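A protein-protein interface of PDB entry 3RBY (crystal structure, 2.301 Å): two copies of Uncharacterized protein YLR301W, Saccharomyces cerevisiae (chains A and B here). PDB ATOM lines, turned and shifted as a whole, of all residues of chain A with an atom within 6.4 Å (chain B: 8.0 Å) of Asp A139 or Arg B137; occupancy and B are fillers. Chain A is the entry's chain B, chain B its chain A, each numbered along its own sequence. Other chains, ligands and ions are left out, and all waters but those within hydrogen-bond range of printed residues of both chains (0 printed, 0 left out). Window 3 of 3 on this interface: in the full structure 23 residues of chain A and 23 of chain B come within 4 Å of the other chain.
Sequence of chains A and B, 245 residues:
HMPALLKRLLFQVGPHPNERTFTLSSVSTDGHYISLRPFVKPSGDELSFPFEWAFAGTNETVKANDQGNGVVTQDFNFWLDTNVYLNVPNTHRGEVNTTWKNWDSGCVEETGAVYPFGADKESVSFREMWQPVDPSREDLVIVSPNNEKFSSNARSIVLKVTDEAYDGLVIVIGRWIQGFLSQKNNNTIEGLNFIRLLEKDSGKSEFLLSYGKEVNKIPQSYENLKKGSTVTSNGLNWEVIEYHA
The guanidinium group (NH1) of Arg A137 is in salt-bridge range of the side-chain carboxylate (OD2) of Asp B139 (3.0 Å). The backbone NH (N) of Ile B142 sits at hydrogen-bond distance from the backbone carbonyl oxygen (O) of Leu A140 (2.8 Å). The guanidinium group of Arg B137 is in salt-bridge range of the side-chain carboxylate of Asp A139, at 2.5 Å.
NH2 of Arg B137 lies within salt-bridge range of OD2 of Asp B134 (3.6 Å). N of Asp A134 is in hydrogen-bond range of O of Val A141, 2.9 Å away. The indole nitrogen (NE1) of Trp A176 sits at hydrogen-bond distance from the backbone carbonyl oxygen (O) of Arg A137 (2.8 Å). The backbone carbonyl oxygen (O) of Arg B137 sits at hydrogen-bond distance from the indole nitrogen (NE1) of Trp B176. The backbone carbonyl oxygen (O) of Val B141 lies within hydrogen-bond range of the backbone NH (N) of Asp B134 (3.1 Å).
Among the printed residues, pairs that only touch across the chains: Leu A140 with Val B141, Val A141 with Leu B140, Leu A140 with Pro B145, Val A141 with Asp B139 and Leu A140 with Leu B140.
Of chain B, only Arg B137 (2.5 Å) comes within 4 Å of Asp A139. Arg B137 touches one residue of chain A. Printed residues of chain A within 4 Å of Ile B142: Leu A140. Printed residues of chain A within 4 Å of Pro B145: Leu A140 (3.6 Å). Ser B136 touches none of the printed residues of chain A. The nearest residue of chain A that does not touch Arg B137 is Arg A137 (5.6 Å).
Hydrophobic or aromatic side chains of chain A that line the printed part of chain B: Leu A140 and Val A141. Among the printed residues, Asp or Glu carboxylates within 4 Å of a Lys or Arg side-chain nitrogen of the other chain: Arg A137 with Asp B139 and Asp A139 with Arg B137.
Arg A137 touches Asp B139, and with the chains exchanged Asp A139 touches Arg B137. Leu A140 touches its own counterpart, Leu B140. Leu A140 touches Val B141, and with the chains exchanged Val A141 touches Leu B140. Val A141 touches Asp B139, but with the chains exchanged Asp A139 does not touch Val B141 (4.5 Å). Positions printed for both chains: 133, 134, 136, 137, 138, 139, 140, 141, 176, 198 and 201. Of the 8 pairs that touch across the chains among the printed residues, 5 have their exchanged pair printed and touching as well.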
ATOM      1  N   VAL A 133       6.325  32.532  13.954  1.00  0.00           N
ATOM      2  CA  VAL A 133       7.643  31.908  14.005  1.00  0.00           C
ATOM      3  C   VAL A 133       8.733  32.972  14.200  1.00  0.00           C
ATOM      4  O   VAL A 133       8.494  34.154  13.978  1.00  0.00           O
ATOM      5  CB  VAL A 133       7.944  31.105  12.695  1.00  0.00           C
ATOM      6  CG1 VAL A 133       7.154  29.782  12.647  1.00  0.00           C
ATOM      7  CG2 VAL A 133       7.659  31.961  11.474  1.00  0.00           C
ATOM      8  N   ASP A 134       9.937  32.556  14.589  1.00  0.00           N
ATOM      9  CA  ASP A 134      11.021  33.504  14.855  1.00  0.00           C
ATOM     10  C   ASP A 134      11.822  33.866  13.592  1.00  0.00           C
ATOM     11  O   ASP A 134      12.682  33.099  13.149  1.00  0.00           O
ATOM     12  CB  ASP A 134      11.938  32.961  15.962  1.00  0.00           C
ATOM     13  CG  ASP A 134      13.139  33.874  16.252  1.00  0.00           C
ATOM     14  OD1 ASP A 134      13.932  33.533  17.157  1.00  0.00           O
ATOM     15  OD2 ASP A 134      13.304  34.920  15.578  1.00  0.00           O
ATOM     16  N   SER A 136      14.266  35.511  12.954  1.00  0.00           N
ATOM     17  CA  SER A 136      15.725  35.588  13.039  1.00  0.00           C
ATOM     18  C   SER A 136      16.381  34.215  12.873  1.00  0.00           C
ATOM     19  O   SER A 136      17.616  34.093  12.864  1.00  0.00           O
ATOM     20  CB  SER A 136      16.167  36.253  14.346  1.00  0.00           C
ATOM     21  OG  SER A 136      15.904  35.433  15.473  1.00  0.00           O
ATOM     22  N   ARG A 137      15.549  33.188  12.704  1.00  0.00           N
ATOM     23  CA  ARG A 137      16.025  31.812  12.554  1.00  0.00           C
ATOM     24  C   ARG A 137      15.871  31.313  11.115  1.00  0.00           C
ATOM     25  O   ARG A 137      14.902  31.662  10.435  1.00  0.00           O
ATOM     26  CB  ARG A 137      15.246  30.913  13.511  1.00  0.00           C
ATOM     27  CG  ARG A 137      15.392  31.334  14.964  1.00  0.00           C
ATOM     28  CD  ARG A 137      16.821  31.070  15.436  1.00  0.00           C
ATOM     29  NE  ARG A 137      17.056  29.637  15.596  1.00  0.00           N
ATOM     30  CZ  ARG A 137      16.860  28.988  16.742  1.00  0.00           C
ATOM     31  NH1 ARG A 137      16.441  29.668  17.807  1.00  0.00           N
ATOM     32  NH2 ARG A 137      17.081  27.675  16.828  1.00  0.00           N
ATOM     33  N   GLU A 138      16.834  30.520  10.643  1.00  0.00           N
ATOM     34  CA  GLU A 138      16.758  29.986   9.280  1.00  0.00           C
ATOM     35  C   GLU A 138      15.784  28.806   9.217  1.00  0.00           C
ATOM     36  O   GLU A 138      15.296  28.460   8.144  1.00  0.00           O
ATOM     37  CB  GLU A 138      18.125  29.584   8.759  1.00  0.00           C
ATOM     38  CG  GLU A 138      18.742  28.414   9.501  1.00  0.00           C
ATOM     39  CD  GLU A 138      20.047  27.940   8.866  1.00  0.00           C
ATOM     40  OE1 GLU A 138      20.594  26.931   9.362  1.00  0.00           O
ATOM     41  OE2 GLU A 138      20.517  28.564   7.880  1.00  0.00           O
ATOM     42  N   ASP A 139      15.497  28.202  10.370  1.00  0.00           N
ATOM     43  CA  ASP A 139      14.430  27.208  10.454  1.00  0.00           C
ATOM     44  C   ASP A 139      13.118  27.892  10.847  1.00  0.00           C
ATOM     45  O   ASP A 139      13.135  28.994  11.387  1.00  0.00           O
ATOM     46  CB  ASP A 139      14.753  26.153  11.511  1.00  0.00           C
ATOM     47  CG  ASP A 139      16.072  25.459  11.266  1.00  0.00           C
ATOM     48  OD1 ASP A 139      17.003  25.637  12.084  1.00  0.00           O
ATOM     49  OD2 ASP A 139      16.174  24.732  10.254  1.00  0.00           O
ATOM     50  N   LEU A 140      11.995  27.233  10.573  1.00  0.00           N
ATOM     51  CA  LEU A 140      10.699  27.614  11.135  1.00  0.00           C
ATOM     52  C   LEU A 140      10.645  27.207  12.621  1.00  0.00           C
ATOM     53  O   LEU A 140      10.427  26.032  12.969  1.00  0.00           O
ATOM     54  CB  LEU A 140       9.551  26.937  10.371  1.00  0.00           C
ATOM     55  CG  LEU A 140       9.290  27.429   8.951  1.00  0.00           C
ATOM     56  CD1 LEU A 140       8.245  26.549   8.319  1.00  0.00           C
ATOM     57  CD2 LEU A 140       8.825  28.881   8.955  1.00  0.00           C
ATOM     58  N   VAL A 141      10.857  28.186  13.488  1.00  0.00           N
ATOM     59  CA  VAL A 141      10.912  27.980  14.921  1.00  0.00           C
ATOM     60  C   VAL A 141       9.698  28.624  15.584  1.00  0.00           C
ATOM     61  O   VAL A 141       9.519  29.850  15.541  1.00  0.00           O
ATOM     62  CB  VAL A 141      12.141  28.646  15.511  1.00  0.00           C
ATOM     63  CG1 VAL A 141      12.047  28.677  17.054  1.00  0.00           C
ATOM     64  CG2 VAL A 141      13.424  27.977  14.997  1.00  0.00           C
ATOM     65  N   TRP A 176      13.955  36.175   6.527  1.00  0.00           N
ATOM     66  CA  TRP A 176      12.937  35.794   5.546  1.00  0.00           C
ATOM     67  C   TRP A 176      12.503  36.936   4.622  1.00  0.00           C
ATOM     68  O   TRP A 176      12.047  38.001   5.084  1.00  0.00           O
ATOM     69  CB  TRP A 176      11.728  35.202   6.268  1.00  0.00           C
ATOM     70  CG  TRP A 176      12.115  33.996   7.089  1.00  0.00           C
ATOM     71  CD1 TRP A 176      12.771  34.004   8.283  1.00  0.00           C
ATOM     72  CD2 TRP A 176      11.896  32.615   6.757  1.00  0.00           C
ATOM     73  NE1 TRP A 176      12.964  32.720   8.724  1.00  0.00           N
ATOM     74  CE2 TRP A 176      12.439  31.844   7.812  1.00  0.00           C
ATOM     75  CE3 TRP A 176      11.290  31.954   5.680  1.00  0.00           C
ATOM     76  CZ2 TRP A 176      12.403  30.431   7.818  1.00  0.00           C
ATOM     77  CZ3 TRP A 176      11.253  30.543   5.689  1.00  0.00           C
ATOM     78  CH2 TRP A 176      11.803  29.810   6.755  1.00  0.00           C
ATOM     79  N   LEU A 198      15.693  33.077   1.648  1.00  0.00           N
ATOM     80  CA  LEU A 198      16.054  32.760   3.015  1.00  0.00           C
ATOM     81  C   LEU A 198      17.546  32.946   3.157  1.00  0.00           C
ATOM     82  O   LEU A 198      18.311  32.249   2.494  1.00  0.00           O
ATOM     83  CB  LEU A 198      15.704  31.309   3.342  1.00  0.00           C
ATOM     84  CG  LEU A 198      16.140  30.844   4.740  1.00  0.00           C
ATOM     85  CD1 LEU A 198      15.386  31.632   5.802  1.00  0.00           C
ATOM     86  CD2 LEU A 198      15.949  29.328   4.944  1.00  0.00           C
ATOM     87  N   ASP A 201      22.531  30.605   7.810  1.00  0.00           N
ATOM     88  CA  ASP A 201      23.511  30.964   8.833  1.00  0.00           C
ATOM     89  C   ASP A 201      24.853  31.301   8.194  1.00  0.00           C
ATOM     90  O   ASP A 201      25.596  32.147   8.699  1.00  0.00           O
ATOM     91  CB  ASP A 201      23.682  29.832   9.853  1.00  0.00           C
ATOM     92  CG  ASP A 201      22.523  29.743  10.831  1.00  0.00           C
ATOM     93  OD1 ASP A 201      21.670  30.662  10.840  1.00  0.00           O
ATOM     94  OD2 ASP A 201      22.474  28.750  11.597  1.00  0.00           O
ATOM     95  N   LEU B   5       7.776  13.295  17.593  1.00  0.00           N
ATOM     96  CA  LEU B   5       7.427  14.278  18.611  1.00  0.00           C
ATOM     97  C   LEU B   5       6.415  15.233  17.984  1.00  0.00           C
ATOM     98  O   LEU B   5       6.758  15.985  17.074  1.00  0.00           O
ATOM     99  CB  LEU B   5       8.672  15.073  18.996  1.00  0.00           C
ATOM    100  CG  LEU B   5       8.917  15.534  20.437  1.00  0.00           C
ATOM    101  CD1 LEU B   5       9.629  16.880  20.457  1.00  0.00           C
ATOM    102  CD2 LEU B   5       7.645  15.596  21.244  1.00  0.00           C
ATOM    103  N   VAL B 133       7.527  17.956  14.952  1.00  0.00           N
ATOM    104  CA  VAL B 133       8.565  18.880  15.346  1.00  0.00           C
ATOM    105  C   VAL B 133       9.896  18.093  15.407  1.00  0.00           C
ATOM    106  O   VAL B 133       9.886  16.853  15.465  1.00  0.00           O
ATOM    107  CB  VAL B 133       8.102  19.557  16.673  1.00  0.00           C
ATOM    108  CG1 VAL B 133       8.945  19.169  17.865  1.00  0.00           C
ATOM    109  CG2 VAL B 133       7.984  21.069  16.508  1.00  0.00           C
ATOM    110  N   ASP B 134      11.030  18.783  15.354  1.00  0.00           N
ATOM    111  CA  ASP B 134      12.326  18.102  15.267  1.00  0.00           C
ATOM    112  C   ASP B 134      12.906  17.927  16.663  1.00  0.00           C
ATOM    113  O   ASP B 134      13.365  18.899  17.280  1.00  0.00           O
ATOM    114  CB  ASP B 134      13.300  18.883  14.382  1.00  0.00           C
ATOM    115  CG  ASP B 134      14.694  18.247  14.323  1.00  0.00           C
ATOM    116  OD1 ASP B 134      15.010  17.399  15.186  1.00  0.00           O
ATOM    117  OD2 ASP B 134      15.483  18.606  13.418  1.00  0.00           O
ATOM    118  N   PRO B 135      12.883  16.682  17.167  1.00  0.00           N
ATOM    119  CA  PRO B 135      13.223  16.386  18.567  1.00  0.00           C
ATOM    120  C   PRO B 135      14.684  16.608  18.883  1.00  0.00           C
ATOM    121  O   PRO B 135      15.052  16.653  20.056  1.00  0.00           O
ATOM    122  CB  PRO B 135      12.868  14.894  18.719  1.00  0.00           C
ATOM    123  CG  PRO B 135      12.825  14.354  17.333  1.00  0.00           C
ATOM    124  CD  PRO B 135      12.361  15.496  16.463  1.00  0.00           C
ATOM    125  N   SER B 136      15.508  16.739  17.855  1.00  0.00           N
ATOM    126  CA  SER B 136      16.930  16.951  18.079  1.00  0.00           C
ATOM    127  C   SER B 136      17.280  18.424  18.315  1.00  0.00           C
ATOM    128  O   SER B 136      18.449  18.736  18.524  1.00  0.00           O
ATOM    129  CB  SER B 136      17.758  16.364  16.942  1.00  0.00           C
ATOM    130  OG  SER B 136      17.416  16.948  15.698  1.00  0.00           O
ATOM    131  N   ARG B 137      16.273  19.310  18.308  1.00  0.00           N
ATOM    132  CA  ARG B 137      16.473  20.739  18.612  1.00  0.00           C
ATOM    133  C   ARG B 137      15.955  21.099  19.994  1.00  0.00           C
ATOM    134  O   ARG B 137      14.981  20.499  20.468  1.00  0.00           O
ATOM    135  CB  ARG B 137      15.730  21.608  17.600  1.00  0.00           C
ATOM    136  CG  ARG B 137      15.864  21.089  16.195  1.00  0.00           C
ATOM    137  CD  ARG B 137      17.303  21.172  15.768  1.00  0.00           C
ATOM    138  NE  ARG B 137      17.542  22.393  15.012  1.00  0.00           N
ATOM    139  CZ  ARG B 137      17.796  22.415  13.702  1.00  0.00           C
ATOM    140  NH1 ARG B 137      17.980  23.578  13.091  1.00  0.00           N
ATOM    141  NH2 ARG B 137      17.875  21.276  13.004  1.00  0.00           N
ATOM    142  N   GLU B 138      16.574  22.094  20.633  1.00  0.00           N
ATOM    143  CA  GLU B 138      16.057  22.587  21.917  1.00  0.00           C
ATOM    144  C   GLU B 138      14.873  23.558  21.757  1.00  0.00           C
ATOM    145  O   GLU B 138      14.115  23.785  22.703  1.00  0.00           O
ATOM    146  CB  GLU B 138      17.164  23.194  22.778  1.00  0.00           C
ATOM    147  CG  GLU B 138      17.513  24.648  22.477  1.00  0.00           C
ATOM    148  CD  GLU B 138      18.642  25.160  23.370  1.00  0.00           C
ATOM    149  OE1 GLU B 138      18.858  26.389  23.417  1.00  0.00           O
ATOM    150  OE2 GLU B 138      19.320  24.329  24.021  1.00  0.00           O
ATOM    151  N   ASP B 139      14.708  24.113  20.561  1.00  0.00           N
ATOM    152  CA  ASP B 139      13.512  24.887  20.237  1.00  0.00           C
ATOM    153  C   ASP B 139      12.465  24.006  19.537  1.00  0.00           C
ATOM    154  O   ASP B 139      12.755  22.889  19.098  1.00  0.00           O
ATOM    155  CB  ASP B 139      13.893  26.053  19.326  1.00  0.00           C
ATOM    156  CG  ASP B 139      14.749  27.079  20.028  1.00  0.00           C
ATOM    157  OD1 ASP B 139      14.295  27.627  21.062  1.00  0.00           O
ATOM    158  OD2 ASP B 139      15.874  27.325  19.552  1.00  0.00           O
ATOM    159  N   LEU B 140      11.255  24.537  19.412  1.00  0.00           N
ATOM    160  CA  LEU B 140      10.190  23.863  18.684  1.00  0.00           C
ATOM    161  C   LEU B 140      10.253  24.241  17.208  1.00  0.00           C
ATOM    162  O   LEU B 140       9.678  25.247  16.795  1.00  0.00           O
ATOM    163  CB  LEU B 140       8.826  24.245  19.260  1.00  0.00           C
ATOM    164  CG  LEU B 140       8.172  23.253  20.221  1.00  0.00           C
ATOM    165  CD1 LEU B 140       9.179  22.739  21.236  1.00  0.00           C
ATOM    166  CD2 LEU B 140       6.984  23.896  20.917  1.00  0.00           C
ATOM    167  N   VAL B 141      10.956  23.438  16.417  1.00  0.00           N
ATOM    168  CA  VAL B 141      11.100  23.714  14.992  1.00  0.00           C
ATOM    169  C   VAL B 141      10.207  22.813  14.145  1.00  0.00           C
ATOM    170  O   VAL B 141      10.198  21.594  14.312  1.00  0.00           O
ATOM    171  CB  VAL B 141      12.561  23.569  14.525  1.00  0.00           C
ATOM    172  CG1 VAL B 141      13.488  23.410  15.719  1.00  0.00           C
ATOM    173  CG2 VAL B 141      12.699  22.394  13.571  1.00  0.00           C
ATOM    174  N   ILE B 142       9.460  23.425  13.233  1.00  0.00           N
ATOM    175  CA  ILE B 142       8.554  22.693  12.357  1.00  0.00           C
ATOM    176  C   ILE B 142       9.321  21.815  11.374  1.00  0.00           C
ATOM    177  O   ILE B 142      10.368  22.208  10.862  1.00  0.00           O
ATOM    178  CB  ILE B 142       7.637  23.650  11.574  1.00  0.00           C
ATOM    179  CG1 ILE B 142       6.538  24.196  12.487  1.00  0.00           C
ATOM    180  CG2 ILE B 142       7.037  22.946  10.369  1.00  0.00           C
ATOM    181  CD1 ILE B 142       6.085  25.593  12.129  1.00  0.00           C
ATOM    182  N   VAL B 143       8.793  20.623  11.117  1.00  0.00           N
ATOM    183  CA  VAL B 143       9.440  19.676  10.215  1.00  0.00           C
ATOM    184  C   VAL B 143       8.641  19.621   8.919  1.00  0.00           C
ATOM    185  O   VAL B 143       7.409  19.576   8.966  1.00  0.00           O
ATOM    186  CB  VAL B 143       9.463  18.266  10.861  1.00  0.00           C
ATOM    187  CG1 VAL B 143       9.273  17.161   9.823  1.00  0.00           C
ATOM    188  CG2 VAL B 143      10.734  18.056  11.672  1.00  0.00           C
ATOM    189  N   PRO B 145       7.574  21.649   6.236  1.00  0.00           N
ATOM    190  CA  PRO B 145       6.432  22.508   5.885  1.00  0.00           C
ATOM    191  C   PRO B 145       6.089  22.383   4.407  1.00  0.00           C
ATOM    192  O   PRO B 145       4.980  22.739   3.998  1.00  0.00           O
ATOM    193  CB  PRO B 145       6.968  23.917   6.151  1.00  0.00           C
ATOM    194  CG  PRO B 145       8.476  23.790   5.972  1.00  0.00           C
ATOM    195  CD  PRO B 145       8.796  22.430   6.527  1.00  0.00           C
ATOM    196  N   PHE B 150      12.414  14.358   5.817  1.00  0.00           N
ATOM    197  CA  PHE B 150      12.960  14.570   7.152  1.00  0.00           C
ATOM    198  C   PHE B 150      13.497  13.278   7.735  1.00  0.00           C
ATOM    199  O   PHE B 150      12.791  12.267   7.797  1.00  0.00           O
ATOM    200  CB  PHE B 150      11.923  15.160   8.104  1.00  0.00           C
ATOM    201  CG  PHE B 150      12.445  15.358   9.496  1.00  0.00           C
ATOM    202  CD1 PHE B 150      12.034  14.526  10.528  1.00  0.00           C
ATOM    203  CD2 PHE B 150      13.371  16.357   9.771  1.00  0.00           C
ATOM    204  CE1 PHE B 150      12.531  14.689  11.819  1.00  0.00           C
ATOM    205  CE2 PHE B 150      13.874  16.529  11.066  1.00  0.00           C
ATOM    206  CZ  PHE B 150      13.455  15.692  12.089  1.00  0.00           C
ATOM    207  N   SER B 152      15.759  11.909  11.238  1.00  0.00           N
ATOM    208  CA  SER B 152      16.362  12.284  12.513  1.00  0.00           C
ATOM    209  C   SER B 152      17.250  11.162  13.029  1.00  0.00           C
ATOM    210  O   SER B 152      16.837   9.995  13.077  1.00  0.00           O
ATOM    211  CB  SER B 152      15.295  12.656  13.554  1.00  0.00           C
ATOM    212  OG  SER B 152      15.785  13.654  14.437  1.00  0.00           O
ATOM    213  N   ALA B 154      17.809  11.171  15.906  1.00  0.00           N
ATOM    214  CA  ALA B 154      17.383  11.361  17.287  1.00  0.00           C
ATOM    215  C   ALA B 154      17.263  10.039  18.026  1.00  0.00           C
ATOM    216  O   ALA B 154      16.590   9.107  17.569  1.00  0.00           O
ATOM    217  CB  ALA B 154      16.075  12.122  17.361  1.00  0.00           C
ATOM    218  N   ILE B 173      12.953  11.259  23.466  1.00  0.00           N
ATOM    219  CA  ILE B 173      13.142  11.458  22.032  1.00  0.00           C
ATOM    220  C   ILE B 173      14.028  12.671  21.744  1.00  0.00           C
ATOM    221  O   ILE B 173      13.640  13.840  21.983  1.00  0.00           O
ATOM    222  CB  ILE B 173      11.808  11.609  21.298  1.00  0.00           C
ATOM    223  CG1 ILE B 173      10.878  10.447  21.675  1.00  0.00           C
ATOM    224  CG2 ILE B 173      12.045  11.675  19.781  1.00  0.00           C
ATOM    225  CD1 ILE B 173       9.521  10.520  21.004  1.00  0.00           C
ATOM    226  N   GLY B 174      15.213  12.395  21.210  1.00  0.00           N
ATOM    227  CA  GLY B 174      16.201  13.439  21.031  1.00  0.00           C
ATOM    228  C   GLY B 174      16.426  14.180  22.336  1.00  0.00           C
ATOM    229  O   GLY B 174      16.797  13.559  23.356  1.00  0.00           O
ATOM    230  N   ARG B 175      16.181  15.493  22.320  1.00  0.00           N
ATOM    231  CA  ARG B 175      16.395  16.318  23.502  1.00  0.00           C
ATOM    232  C   ARG B 175      15.195  16.362  24.442  1.00  0.00           C
ATOM    233  O   ARG B 175      15.298  16.868  25.564  1.00  0.00           O
ATOM    234  CB  ARG B 175      16.779  17.735  23.095  1.00  0.00           C
ATOM    235  CG  ARG B 175      18.144  17.848  22.410  1.00  0.00           C
ATOM    236  CD  ARG B 175      18.384  19.304  22.048  1.00  0.00           C
ATOM    237  NE  ARG B 175      19.754  19.735  22.304  1.00  0.00           N
ATOM    238  CZ  ARG B 175      20.781  19.355  21.560  1.00  0.00           C
ATOM    239  NH1 ARG B 175      20.585  18.526  20.539  1.00  0.00           N
ATOM    240  NH2 ARG B 175      22.000  19.790  21.845  1.00  0.00           N
ATOM    241  N   TRP B 176      14.066  15.815  23.999  1.00  0.00           N
ATOM    242  CA  TRP B 176      12.804  15.983  24.735  1.00  0.00           C
ATOM    243  C   TRP B 176      12.353  14.739  25.511  1.00  0.00           C
ATOM    244  O   TRP B 176      12.097  13.679  24.927  1.00  0.00           O
ATOM    245  CB  TRP B 176      11.685  16.411  23.788  1.00  0.00           C
ATOM    246  CG  TRP B 176      11.909  17.734  23.127  1.00  0.00           C
ATOM    247  CD1 TRP B 176      12.691  17.980  22.036  1.00  0.00           C
ATOM    248  CD2 TRP B 176      11.319  19.002  23.495  1.00  0.00           C
ATOM    249  NE1 TRP B 176      12.641  19.319  21.710  1.00  0.00           N
ATOM    250  CE2 TRP B 176      11.807  19.969  22.586  1.00  0.00           C
ATOM    251  CE3 TRP B 176      10.445  19.409  24.509  1.00  0.00           C
ATOM    252  CZ2 TRP B 176      11.438  21.334  22.657  1.00  0.00           C
ATOM    253  CZ3 TRP B 176      10.071  20.766  24.581  1.00  0.00           C
ATOM    254  CH2 TRP B 176      10.567  21.707  23.661  1.00  0.00           C
ATOM    255  N   LEU B 198      14.112  18.933  29.231  1.00  0.00           N
ATOM    256  CA  LEU B 198      14.751  19.293  27.975  1.00  0.00           C
ATOM    257  C   LEU B 198      16.255  19.350  28.167  1.00  0.00           C
ATOM    258  O   LEU B 198      16.747  20.068  29.050  1.00  0.00           O
ATOM    259  CB  LEU B 198      14.218  20.641  27.470  1.00  0.00           C
ATOM    260  CG  LEU B 198      14.785  21.238  26.171  1.00  0.00           C
ATOM    261  CD1 LEU B 198      14.424  20.382  24.964  1.00  0.00           C
ATOM    262  CD2 LEU B 198      14.275  22.676  25.978  1.00  0.00           C
ATOM    263  N   GLU B 199      16.987  18.579  27.365  1.00  0.00           N
ATOM    264  CA  GLU B 199      18.446  18.690  27.349  1.00  0.00           C
ATOM    265  C   GLU B 199      18.845  19.776  26.350  1.00  0.00           C
ATOM    266  O   GLU B 199      18.708  19.606  25.136  1.00  0.00           O
ATOM    267  CB  GLU B 199      19.134  17.362  27.015  1.00  0.00           C
ATOM    268  CG  GLU B 199      20.641  17.529  26.761  1.00  0.00           C
ATOM    269  CD  GLU B 199      21.364  16.214  26.462  1.00  0.00           C
ATOM    270  OE1 GLU B 199      22.302  16.210  25.620  1.00  0.00           O
ATOM    271  OE2 GLU B 199      21.003  15.184  27.078  1.00  0.00           O
ATOM    272  N   LYS B 200      19.319  20.894  26.892  1.00  0.00           N
ATOM    273  CA  LYS B 200      19.709  22.074  26.132  1.00  0.00           C
ATOM    274  C   LYS B 200      21.042  21.849  25.431  1.00  0.00           C
ATOM    275  O   LYS B 200      21.837  21.003  25.858  1.00  0.00           O
ATOM    276  CB  LYS B 200      19.868  23.270  27.087  1.00  0.00           C
ATOM    277  CG  LYS B 200      18.621  23.666  27.854  1.00  0.00           C
ATOM    278  CD  LYS B 200      17.625  24.376  26.957  1.00  0.00           C
ATOM    279  CE  LYS B 200      16.961  25.539  27.675  1.00  0.00           C
ATOM    280  NZ  LYS B 200      17.911  26.665  27.899  1.00  0.00           N
ATOM    281  N   ASP B 201      21.296  22.620  24.374  1.00  0.00           N
ATOM    282  CA  ASP B 201      22.582  22.567  23.680  1.00  0.00           C
ATOM    283  C   ASP B 201      23.760  22.781  24.640  1.00  0.00           C
ATOM    284  O   ASP B 201      24.868  22.333  24.364  1.00  0.00           O
ATOM    285  CB  ASP B 201      22.641  23.591  22.537  1.00  0.00           C
ATOM    286  CG  ASP B 201      21.499  23.432  21.532  1.00  0.00           C
ATOM    287  OD1 ASP B 201      20.837  22.370  21.514  1.00  0.00           O
ATOM    288  OD2 ASP B 201      21.269  24.386  20.750  1.00  0.00           O
